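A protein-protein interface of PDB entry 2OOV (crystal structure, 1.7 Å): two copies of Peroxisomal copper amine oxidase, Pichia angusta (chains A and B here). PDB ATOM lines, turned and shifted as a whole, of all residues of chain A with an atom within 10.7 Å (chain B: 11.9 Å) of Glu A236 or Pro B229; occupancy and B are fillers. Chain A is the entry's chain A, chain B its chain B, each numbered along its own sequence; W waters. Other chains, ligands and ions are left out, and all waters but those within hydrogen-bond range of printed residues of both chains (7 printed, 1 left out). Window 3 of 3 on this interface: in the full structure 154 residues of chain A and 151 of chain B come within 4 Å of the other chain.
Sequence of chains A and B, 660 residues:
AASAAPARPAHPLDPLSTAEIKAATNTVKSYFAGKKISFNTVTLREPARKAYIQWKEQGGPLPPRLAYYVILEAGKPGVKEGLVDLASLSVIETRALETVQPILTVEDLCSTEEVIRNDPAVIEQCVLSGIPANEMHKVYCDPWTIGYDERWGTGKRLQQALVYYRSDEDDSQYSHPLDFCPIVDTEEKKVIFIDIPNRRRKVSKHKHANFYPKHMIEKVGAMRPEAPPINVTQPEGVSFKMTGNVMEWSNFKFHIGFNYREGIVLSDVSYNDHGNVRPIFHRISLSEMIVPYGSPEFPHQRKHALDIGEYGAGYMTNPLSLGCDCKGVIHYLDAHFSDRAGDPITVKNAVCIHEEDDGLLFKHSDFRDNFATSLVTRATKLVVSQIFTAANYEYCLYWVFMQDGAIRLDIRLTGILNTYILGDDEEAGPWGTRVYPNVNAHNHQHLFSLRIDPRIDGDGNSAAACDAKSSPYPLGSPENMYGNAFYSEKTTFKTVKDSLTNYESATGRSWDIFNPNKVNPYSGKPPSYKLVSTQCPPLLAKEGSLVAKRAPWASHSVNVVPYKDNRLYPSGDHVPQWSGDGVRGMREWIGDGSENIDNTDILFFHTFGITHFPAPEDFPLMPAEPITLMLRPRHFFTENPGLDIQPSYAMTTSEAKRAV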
ATOM      1  N   ASN A 231      24.033 -19.049  13.504  1.00  0.00           N
ATOM      2  CA  ASN A 231      25.190 -18.635  14.301  1.00  0.00           C
ATOM      3  C   ASN A 231      25.035 -19.017  15.761  1.00  0.00           C
ATOM      4  O   ASN A 231      24.001 -18.747  16.361  1.00  0.00           O
ATOM      5  CB  ASN A 231      25.418 -17.120  14.183  1.00  0.00           C
ATOM      6  CG  ASN A 231      25.834 -16.696  12.789  1.00  0.00           C
ATOM      7  OD1 ASN A 231      26.460 -17.461  12.050  1.00  0.00           O
ATOM      8  ND2 ASN A 231      25.491 -15.461  12.423  1.00  0.00           N
ATOM      9  N   VAL A 232      26.072 -19.640  16.315  1.00  0.00           N
ATOM     10  CA  VAL A 232      26.097 -20.074  17.708  1.00  0.00           C
ATOM     11  C   VAL A 232      27.135 -19.236  18.450  1.00  0.00           C
ATOM     12  O   VAL A 232      28.301 -19.187  18.049  1.00  0.00           O
ATOM     13  CB  VAL A 232      26.478 -21.583  17.819  1.00  0.00           C
ATOM     14  CG1 VAL A 232      26.506 -22.034  19.266  1.00  0.00           C
ATOM     15  CG2 VAL A 232      25.512 -22.447  17.017  1.00  0.00           C
ATOM     16  N   THR A 233      26.717 -18.565  19.518  1.00  0.00           N
ATOM     17  CA  THR A 233      27.641 -17.775  20.324  1.00  0.00           C
ATOM     18  C   THR A 233      27.439 -18.029  21.818  1.00  0.00           C
ATOM     19  O   THR A 233      26.340 -18.369  22.257  1.00  0.00           O
ATOM     20  CB  THR A 233      27.482 -16.268  20.047  1.00  0.00           C
ATOM     21  OG1 THR A 233      26.143 -15.874  20.343  1.00  0.00           O
ATOM     22  CG2 THR A 233      27.773 -15.950  18.579  1.00  0.00           C
ATOM     23  N   GLN A 234      28.510 -17.877  22.589  1.00  0.00           N
ATOM     24  CA  GLN A 234      28.425 -17.946  24.041  1.00  0.00           C
ATOM     25  C   GLN A 234      29.124 -16.713  24.598  1.00  0.00           C
ATOM     26  O   GLN A 234      30.276 -16.790  25.024  1.00  0.00           O
ATOM     27  CB  GLN A 234      29.056 -19.241  24.565  1.00  0.00           C
ATOM     28  CG  GLN A 234      28.298 -20.490  24.140  1.00  0.00           C
ATOM     29  CD  GLN A 234      28.768 -21.735  24.870  1.00  0.00           C
ATOM     30  OE1 GLN A 234      29.444 -22.571  24.283  1.00  0.00           O
ATOM     31  NE2 GLN A 234      28.417 -21.859  26.149  1.00  0.00           N
ATOM     32  N   PRO A 235      28.420 -15.562  24.577  1.00  0.00           N
ATOM     33  CA  PRO A 235      28.993 -14.262  24.918  1.00  0.00           C
ATOM     34  C   PRO A 235      29.442 -14.122  26.370  1.00  0.00           C
ATOM     35  O   PRO A 235      30.189 -13.197  26.675  1.00  0.00           O
ATOM     36  CB  PRO A 235      27.844 -13.283  24.619  1.00  0.00           C
ATOM     37  CG  PRO A 235      26.624 -14.085  24.746  1.00  0.00           C
ATOM     38  CD  PRO A 235      26.996 -15.445  24.218  1.00  0.00           C
ATOM     39  N   GLU A 236      28.982 -15.006  27.253  1.00  0.00           N
ATOM     40  CA  GLU A 236      29.448 -15.008  28.642  1.00  0.00           C
ATOM     41  C   GLU A 236      30.350 -16.221  28.929  1.00  0.00           C
ATOM     42  O   GLU A 236      30.614 -16.564  30.086  1.00  0.00           O
ATOM     43  CB  GLU A 236      28.262 -14.936  29.613  1.00  0.00           C
ATOM     44  CG  GLU A 236      27.490 -13.598  29.551  1.00  0.00           C
ATOM     45  CD  GLU A 236      26.120 -13.648  30.233  1.00  0.00           C
ATOM     46  OE1 GLU A 236      25.965 -14.333  31.279  1.00  0.00           O
ATOM     47  OE2 GLU A 236      25.185 -12.987  29.716  1.00  0.00           O
ATOM     48  N   GLY A 237      30.839 -16.857  27.869  1.00  0.00           N
ATOM     49  CA  GLY A 237      31.729 -18.001  28.024  1.00  0.00           C
ATOM     50  C   GLY A 237      30.997 -19.309  28.251  1.00  0.00           C
ATOM     51  O   GLY A 237      29.773 -19.384  28.113  1.00  0.00           O
ATOM     52  N   VAL A 238      31.756 -20.349  28.576  1.00  0.00           N
ATOM     53  CA  VAL A 238      31.196 -21.695  28.722  1.00  0.00           C
ATOM     54  C   VAL A 238      30.955 -22.036  30.187  1.00  0.00           C
ATOM     55  O   VAL A 238      31.522 -21.400  31.084  1.00  0.00           O
ATOM     56  CB  VAL A 238      32.128 -22.769  28.092  1.00  0.00           C
ATOM     57  CG1 VAL A 238      32.372 -22.471  26.628  1.00  0.00           C
ATOM     58  CG2 VAL A 238      33.444 -22.862  28.847  1.00  0.00           C
ATOM     59  N   SER A 239      30.127 -23.053  30.425  1.00  0.00           N
ATOM     60  CA  SER A 239      29.817 -23.471  31.783  1.00  0.00           C
ATOM     61  C   SER A 239      30.807 -24.515  32.307  1.00  0.00           C
ATOM     62  O   SER A 239      30.870 -24.742  33.517  1.00  0.00           O
ATOM     63  CB  SER A 239      28.376 -24.003  31.887  1.00  0.00           C
ATOM     64  OG  SER A 239      28.288 -25.334  31.396  1.00  0.00           O
ATOM     65  N   PHE A 240      31.566 -25.149  31.415  1.00  0.00           N
ATOM     66  CA  PHE A 240      32.535 -26.167  31.845  1.00  0.00           C
ATOM     67  C   PHE A 240      33.870 -25.545  32.265  1.00  0.00           C
ATOM     68  O   PHE A 240      34.229 -24.455  31.801  1.00  0.00           O
ATOM     69  CB  PHE A 240      32.725 -27.278  30.797  1.00  0.00           C
ATOM     70  CG  PHE A 240      33.318 -26.818  29.478  1.00  0.00           C
ATOM     71  CD1 PHE A 240      34.707 -26.741  29.304  1.00  0.00           C
ATOM     72  CD2 PHE A 240      32.494 -26.526  28.398  1.00  0.00           C
ATOM     73  CE1 PHE A 240      35.265 -26.350  28.081  1.00  0.00           C
ATOM     74  CE2 PHE A 240      33.041 -26.120  27.154  1.00  0.00           C
ATOM     75  CZ  PHE A 240      34.436 -26.036  27.005  1.00  0.00           C
ATOM     76  N   GLY A 328      30.977 -23.699  17.220  1.00  0.00           N
ATOM     77  CA  GLY A 328      30.742 -23.032  18.491  1.00  0.00           C
ATOM     78  C   GLY A 328      32.029 -22.623  19.174  1.00  0.00           C
ATOM     79  O   GLY A 328      33.067 -22.441  18.516  1.00  0.00           O
ATOM     80  N   VAL A 329      31.953 -22.455  20.493  1.00  0.00           N
ATOM     81  CA  VAL A 329      33.112 -22.102  21.293  1.00  0.00           C
ATOM     82  C   VAL A 329      33.754 -23.402  21.772  1.00  0.00           C
ATOM     83  O   VAL A 329      33.167 -24.150  22.563  1.00  0.00           O
ATOM     84  CB  VAL A 329      32.739 -21.194  22.491  1.00  0.00           C
ATOM     85  CG1 VAL A 329      33.978 -20.862  23.322  1.00  0.00           C
ATOM     86  CG2 VAL A 329      32.027 -19.901  21.997  1.00  0.00           C
ATOM     87  N   GLU A 355      30.193 -27.498  24.608  1.00  0.00           N
ATOM     88  CA  GLU A 355      28.838 -27.780  25.062  1.00  0.00           C
ATOM     89  C   GLU A 355      27.838 -27.297  24.019  1.00  0.00           C
ATOM     90  O   GLU A 355      28.076 -26.296  23.335  1.00  0.00           O
ATOM     91  CB  GLU A 355      28.576 -27.187  26.455  1.00  0.00           C
ATOM     92  CG  GLU A 355      28.678 -25.677  26.538  1.00  0.00           C
ATOM     93  CD  GLU A 355      28.568 -25.129  27.956  1.00  0.00           C
ATOM     94  OE1 GLU A 355      28.383 -25.903  28.921  1.00  0.00           O
ATOM     95  OE2 GLU A 355      28.684 -23.902  28.113  1.00  0.00           O
ATOM     96  N   GLU A 356      26.738 -28.037  23.884  1.00  0.00           N
ATOM     97  CA  GLU A 356      25.764 -27.841  22.804  1.00  0.00           C
ATOM     98  C   GLU A 356      24.362 -27.897  23.389  1.00  0.00           C
ATOM     99  O   GLU A 356      24.118 -28.634  24.358  1.00  0.00           O
ATOM    100  CB  GLU A 356      25.846 -28.978  21.773  1.00  0.00           C
ATOM    101  CG  GLU A 356      26.965 -28.922  20.746  1.00  0.00           C
ATOM    102  CD  GLU A 356      26.875 -30.074  19.754  1.00  0.00           C
ATOM    103  OE1 GLU A 356      25.868 -30.170  19.011  1.00  0.00           O
ATOM    104  OE2 GLU A 356      27.804 -30.911  19.716  1.00  0.00           O
ATOM    105  N   ASP A 357      23.447 -27.131  22.789  1.00  0.00           N
ATOM    106  CA  ASP A 357      22.015 -27.315  23.032  1.00  0.00           C
ATOM    107  C   ASP A 357      21.653 -28.770  22.745  1.00  0.00           C
ATOM    108  O   ASP A 357      22.121 -29.341  21.756  1.00  0.00           O
ATOM    109  CB  ASP A 357      21.191 -26.446  22.075  1.00  0.00           C
ATOM    110  CG  ASP A 357      21.293 -24.955  22.369  1.00  0.00           C
ATOM    111  OD1 ASP A 357      21.611 -24.575  23.513  1.00  0.00           O
ATOM    112  OD2 ASP A 357      21.010 -24.153  21.440  1.00  0.00           O
ATOM    113  N   ARG A 378      15.456 -26.758  29.654  1.00  0.00           N
ATOM    114  CA  ARG A 378      16.218 -27.144  28.470  1.00  0.00           C
ATOM    115  C   ARG A 378      17.474 -27.899  28.891  1.00  0.00           C
ATOM    116  O   ARG A 378      17.996 -27.692  30.004  1.00  0.00           O
ATOM    117  CB  ARG A 378      16.550 -25.921  27.608  1.00  0.00           C
ATOM    118  CG  ARG A 378      15.277 -25.254  27.011  1.00  0.00           C
ATOM    119  CD  ARG A 378      15.555 -24.347  25.797  1.00  0.00           C
ATOM    120  NE  ARG A 378      16.192 -25.094  24.704  1.00  0.00           N
ATOM    121  CZ  ARG A 378      15.544 -25.732  23.732  1.00  0.00           C
ATOM    122  NH1 ARG A 378      14.216 -25.705  23.664  1.00  0.00           N
ATOM    123  NH2 ARG A 378      16.234 -26.381  22.800  1.00  0.00           N
ATOM    124  N   ALA A 379      17.936 -28.778  27.993  1.00  0.00           N
ATOM    125  CA  ALA A 379      19.114 -29.626  28.203  1.00  0.00           C
ATOM    126  C   ALA A 379      20.331 -29.068  27.483  1.00  0.00           C
ATOM    127  O   ALA A 379      20.217 -28.579  26.359  1.00  0.00           O
ATOM    128  CB  ALA A 379      18.848 -31.039  27.684  1.00  0.00           C
ATOM    129  N   THR A 380      21.475 -29.120  28.151  1.00  0.00           N
ATOM    130  CA  THR A 380      22.753 -28.875  27.505  1.00  0.00           C
ATOM    131  C   THR A 380      23.558 -30.185  27.574  1.00  0.00           C
ATOM    132  O   THR A 380      23.474 -30.902  28.574  1.00  0.00           O
ATOM    133  CB  THR A 380      23.487 -27.705  28.186  1.00  0.00           C
ATOM    134  OG1 THR A 380      22.646 -26.537  28.155  1.00  0.00           O
ATOM    135  CG2 THR A 380      24.828 -27.411  27.476  1.00  0.00           C
ATOM    136  N   SER A 648      13.706 -22.998  31.950  1.00  0.00           N
ATOM    137  CA  SER A 648      13.568 -21.987  30.905  1.00  0.00           C
ATOM    138  C   SER A 648      12.266 -21.210  31.112  1.00  0.00           C
ATOM    139  O   SER A 648      12.185 -20.015  30.824  1.00  0.00           O
ATOM    140  CB  SER A 648      13.576 -22.648  29.529  1.00  0.00           C
ATOM    141  OG  SER A 648      14.818 -23.288  29.303  1.00  0.00           O
ATOM    142  N   PRO B 225      23.227 -21.789  39.720  1.00  0.00           N
ATOM    143  CA  PRO B 225      23.164 -20.474  39.067  1.00  0.00           C
ATOM    144  C   PRO B 225      22.782 -20.647  37.599  1.00  0.00           C
ATOM    145  O   PRO B 225      23.079 -21.695  37.016  1.00  0.00           O
ATOM    146  CB  PRO B 225      24.609 -19.954  39.160  1.00  0.00           C
ATOM    147  CG  PRO B 225      25.290 -20.799  40.185  1.00  0.00           C
ATOM    148  CD  PRO B 225      24.585 -22.121  40.194  1.00  0.00           C
ATOM    149  N   GLU B 226      22.125 -19.646  37.010  1.00  0.00           N
ATOM    150  CA  GLU B 226      21.857 -19.686  35.576  1.00  0.00           C
ATOM    151  C   GLU B 226      23.185 -19.889  34.853  1.00  0.00           C
ATOM    152  O   GLU B 226      24.178 -19.228  35.169  1.00  0.00           O
ATOM    153  CB  GLU B 226      21.157 -18.413  35.089  1.00  0.00           C
ATOM    154  CG  GLU B 226      20.688 -18.462  33.627  1.00  0.00           C
ATOM    155  CD  GLU B 226      19.642 -19.549  33.371  1.00  0.00           C
ATOM    156  OE1 GLU B 226      18.547 -19.477  33.965  1.00  0.00           O
ATOM    157  OE2 GLU B 226      19.909 -20.477  32.571  1.00  0.00           O
ATOM    158  N   ALA B 227      23.202 -20.852  33.934  1.00  0.00           N
ATOM    159  CA  ALA B 227      24.380 -21.140  33.121  1.00  0.00           C
ATOM    160  C   ALA B 227      24.610 -20.016  32.117  1.00  0.00           C
ATOM    161  O   ALA B 227      23.653 -19.350  31.702  1.00  0.00           O
ATOM    162  CB  ALA B 227      24.213 -22.466  32.388  1.00  0.00           C
ATOM    163  N   PRO B 228      25.882 -19.788  31.730  1.00  0.00           N
ATOM    164  CA  PRO B 228      26.104 -18.824  30.653  1.00  0.00           C
ATOM    165  C   PRO B 228      25.392 -19.323  29.394  1.00  0.00           C
ATOM    166  O   PRO B 228      25.426 -20.519  29.106  1.00  0.00           O
ATOM    167  CB  PRO B 228      27.634 -18.819  30.472  1.00  0.00           C
ATOM    168  CG  PRO B 228      28.135 -20.025  31.161  1.00  0.00           C
ATOM    169  CD  PRO B 228      27.140 -20.372  32.232  1.00  0.00           C
ATOM    170  N   PRO B 229      24.720 -18.420  28.663  1.00  0.00           N
ATOM    171  CA  PRO B 229      23.834 -18.865  27.595  1.00  0.00           C
ATOM    172  C   PRO B 229      24.552 -19.355  26.335  1.00  0.00           C
ATOM    173  O   PRO B 229      25.708 -19.008  26.088  1.00  0.00           O
ATOM    174  CB  PRO B 229      23.029 -17.600  27.271  1.00  0.00           C
ATOM    175  CG  PRO B 229      23.986 -16.488  27.564  1.00  0.00           C
ATOM    176  CD  PRO B 229      24.740 -16.948  28.787  1.00  0.00           C
ATOM    177  N   ILE B 230      23.846 -20.174  25.566  1.00  0.00           N
ATOM    178  CA  ILE B 230      24.220 -20.514  24.209  1.00  0.00           C
ATOM    179  C   ILE B 230      23.163 -19.822  23.354  1.00  0.00           C
ATOM    180  O   ILE B 230      21.975 -20.135  23.470  1.00  0.00           O
ATOM    181  CB  ILE B 230      24.144 -22.042  23.963  1.00  0.00           C
ATOM    182  CG1 ILE B 230      25.050 -22.795  24.943  1.00  0.00           C
ATOM    183  CG2 ILE B 230      24.468 -22.380  22.487  1.00  0.00           C
ATOM    184  CD1 ILE B 230      24.818 -24.311  24.957  1.00  0.00           C
ATOM    185  N   ASN B 231      23.586 -18.873  22.521  1.00  0.00           N
ATOM    186  CA  ASN B 231      22.639 -18.092  21.722  1.00  0.00           C
ATOM    187  C   ASN B 231      22.656 -18.504  20.265  1.00  0.00           C
ATOM    188  O   ASN B 231      23.717 -18.550  19.650  1.00  0.00           O
ATOM    189  CB  ASN B 231      22.940 -16.588  21.814  1.00  0.00           C
ATOM    190  CG  ASN B 231      22.778 -16.031  23.217  1.00  0.00           C
ATOM    191  OD1 ASN B 231      21.908 -16.457  23.988  1.00  0.00           O
ATOM    192  ND2 ASN B 231      23.610 -15.049  23.550  1.00  0.00           N
ATOM    193  N   VAL B 232      21.471 -18.780  19.723  1.00  0.00           N
ATOM    194  CA  VAL B 232      21.303 -19.180  18.327  1.00  0.00           C
ATOM    195  C   VAL B 232      20.607 -18.047  17.586  1.00  0.00           C
ATOM    196  O   VAL B 232      19.528 -17.604  17.991  1.00  0.00           O
ATOM    197  CB  VAL B 232      20.426 -20.463  18.204  1.00  0.00           C
ATOM    198  CG1 VAL B 232      20.264 -20.876  16.739  1.00  0.00           C
ATOM    199  CG2 VAL B 232      21.007 -21.607  19.025  1.00  0.00           C
ATOM    200  N   THR B 233      21.223 -17.570  16.508  1.00  0.00           N
ATOM    201  CA  THR B 233      20.630 -16.519  15.696  1.00  0.00           C
ATOM    202  C   THR B 233      20.745 -16.853  14.212  1.00  0.00           C
ATOM    203  O   THR B 233      21.663 -17.556  13.797  1.00  0.00           O
ATOM    204  CB  THR B 233      21.313 -15.159  15.945  1.00  0.00           C
ATOM    205  OG1 THR B 233      22.722 -15.303  15.792  1.00  0.00           O
ATOM    206  CG2 THR B 233      21.021 -14.645  17.364  1.00  0.00           C
ATOM    207  N   GLY B 323      10.230 -18.931  22.429  1.00  0.00           N
ATOM    208  CA  GLY B 323      11.613 -18.883  22.894  1.00  0.00           C
ATOM    209  C   GLY B 323      12.031 -19.944  23.893  1.00  0.00           C
ATOM    210  O   GLY B 323      13.211 -19.997  24.275  1.00  0.00           O
ATOM    211  N   LYS B 327      13.784 -23.508  20.474  1.00  0.00           N
ATOM    212  CA  LYS B 327      14.849 -22.509  20.516  1.00  0.00           C
ATOM    213  C   LYS B 327      15.266 -22.104  19.107  1.00  0.00           C
ATOM    214  O   LYS B 327      15.393 -22.952  18.226  1.00  0.00           O
ATOM    215  CB  LYS B 327      16.038 -23.108  21.277  1.00  0.00           C
ATOM    216  CG  LYS B 327      17.256 -22.217  21.390  1.00  0.00           C
ATOM    217  CD  LYS B 327      18.167 -22.718  22.497  1.00  0.00           C
ATOM    218  CE  LYS B 327      19.329 -21.762  22.683  1.00  0.00           C
ATOM    219  NZ  LYS B 327      20.181 -22.217  23.809  1.00  0.00           N
ATOM    220  N   GLY B 328      15.465 -20.806  18.895  1.00  0.00           N
ATOM    221  CA  GLY B 328      15.905 -20.299  17.593  1.00  0.00           C
ATOM    222  C   GLY B 328      14.865 -19.445  16.902  1.00  0.00           C
ATOM    223  O   GLY B 328      13.978 -18.880  17.556  1.00  0.00           O
HETATM  224  O   HOH W   1      25.995 -23.158  29.344  1.00  0.00           O
HETATM  225  O   HOH W   2      14.639 -26.459  20.358  1.00  0.00           O
HETATM  226  O   HOH W   3      18.873 -23.747  25.951  1.00  0.00           O
HETATM  227  O   HOH W   4      24.324 -16.232  18.011  1.00  0.00           O
HETATM  228  O   HOH W   5      24.275 -13.655  14.267  1.00  0.00           O
HETATM  229  O   HOH W   6      25.285 -13.736  21.666  1.00  0.00           O
HETATM  230  O   HOH W   7      23.597 -16.546  32.158  1.00  0.00           O
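The backbone NH (N) of Asn A231 sits at hydrogen-bond distance from the backbone carbonyl oxygen (O) of Thr B233 (2.8 Å).
O of Thr A233 is in hydrogen-bond range of N of Asn B231.
OD1 of Asp A357 is in salt-bridge range of NZ of Lys B327 (2.8 Å).
O of Asn A231 lies close to O of Asn B231 (3.3 Å).
Pro B229 touches Thr A233.
Thr A233 touches Ile B230.
Pro A235 touches Asn B231.
Pro B228 touches Gly A237.
Val A238 touches Pro B228 (C to CG, 3.6 Å).
Glu A356 touches Ile B230.
Asp A357 touches Ile B230.
CG2 of Val B232 touches OD2 of Asp A357, 3.5 Å away.
Lys B327 touches Arg A378.
Ile B230 touches Thr A380 (CD1 to CG2, 3.99 Å).
Hydrophobic or aromatic side chains of chain B that line the printed part of chain A: Pro B228, Pro B229, Ile B230 and Val B232.
Of the 19 printed residues of chain A, 13 touch a printed residue of chain B.
Printed residues of chain A that touch a printed residue of chain B: Asn A231, Val A232, Thr A233, Gln A234, Pro A235, Glu A236, Gly A237, Val A238, Ser A239, Glu A356, Asp A357, Arg A378 and Thr A380.
Hydrophobic or aromatic side chains of chain A within 4 Å of the printed part of chain B: Val A232 and Pro A235.
Among the printed residues, 22 pairs touch across the chains.
Among the printed residues, Asp or Glu carboxylates within 4 Å of a Lys or Arg side-chain nitrogen of the other chain: Asp A357 with Lys B327 (2.8 Å).
The side-chain amide nitrogen (NE2) of Gln A234 lies within hydrogen-bond range of the backbone carbonyl oxygen (O) of Gly A237.
NE2 of Gln A234 lies within hydrogen-bond range of OE2 of Glu A355 (2.8 Å).
OG of Ser A239 lies within hydrogen-bond range of OE1 of Glu A355 (2.5 Å).
O of Ile B230 lies within hydrogen-bond range of NZ of Lys B327 (2.8 Å).
Asn B231 touches its own counterpart, Asn A231.
Asn A231 touches Val B232, and with the chains exchanged Val A232 touches Asn B231.
Asn A231 touches Thr B233, and with the chains exchanged Thr A233 touches Asn B231.
Positions printed for both chains: 231, 232, 233 and 328.
Glu A236 touches two residues of chain B.
Pro B229 touches just these residues of chain A: Thr A233 (3.9 Å), Gln A234 (3.6 Å) and Glu A236 (3.8 Å).
Gln A234 touches just these residues of chain B: Pro B229 (3.6 Å) and Ile B230 (3.7 Å).
Pro A235 touches just one residue of chain B: Asn B231.
Of chain B, only Pro B228 (3.2 Å) comes within 4 Å of Gly A237.
Of chain B, only Pro B228 (3.6 Å) comes within 4 Å of Val A238.
No residue of chain A comes within 4 Å of Ala B227.
Pro B228 touches four residues of chain A.
Of the printed residues of chain B, Thr A233 touches Pro B229 (3.9 Å), Ile B230 (3.6 Å) and Asn B231 (2.8 Å).
Printed residues of chain B within 4 Å of Asp A357: Ile B230 (3.5 Å), Val B232 (3.5 Å) and Lys B327 (2.8 Å).
Printed residues of chain B within 4 Å of Asn A231: Asn B231, Val B232 and Thr B233.
Printed residues of chain B within 4 Å of Val A232: Ile B230 and Asn B231.
Phe A240 touches none of the printed residues of chain B.
The nearest residue of chain B that does not touch Glu A236 is Ala B227 (5.5 Å).
The nearest residue of chain A that does not touch Pro B229 is Pro A235 (4.2 Å).
Water W6 lies within hydrogen-bond range of the side-chain hydroxyl (OG1) of Thr A233 (2.7 Å) and the side-chain amide nitrogen (ND2) of Asn B231 (2.8 Å).
Water W1 bridges O of Pro B228 (2.7 Å) and OE2 of Glu A355 (3.0 Å).
Water W5 lies within hydrogen-bond range of OG1 of Thr B233 (2.7 Å) and ND2 of Asn A231 (2.9 Å).
Water W4 lies within hydrogen-bond range of OG1 of Thr B233 (2.9 Å), O of Asn B231 (2.9 Å), OG1 of Thr A233 (3.0 Å) and O of Asn A231 (3.0 Å).
Water W2 bridges NH2 of Arg A378 (2.9 Å) and N of Lys B327 (3.1 Å).
Water W3 bridges the side-chain amino group (NZ) of Lys B327 (2.9 Å) and the guanidinium group (NE) of Arg A378 (3.2 Å).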
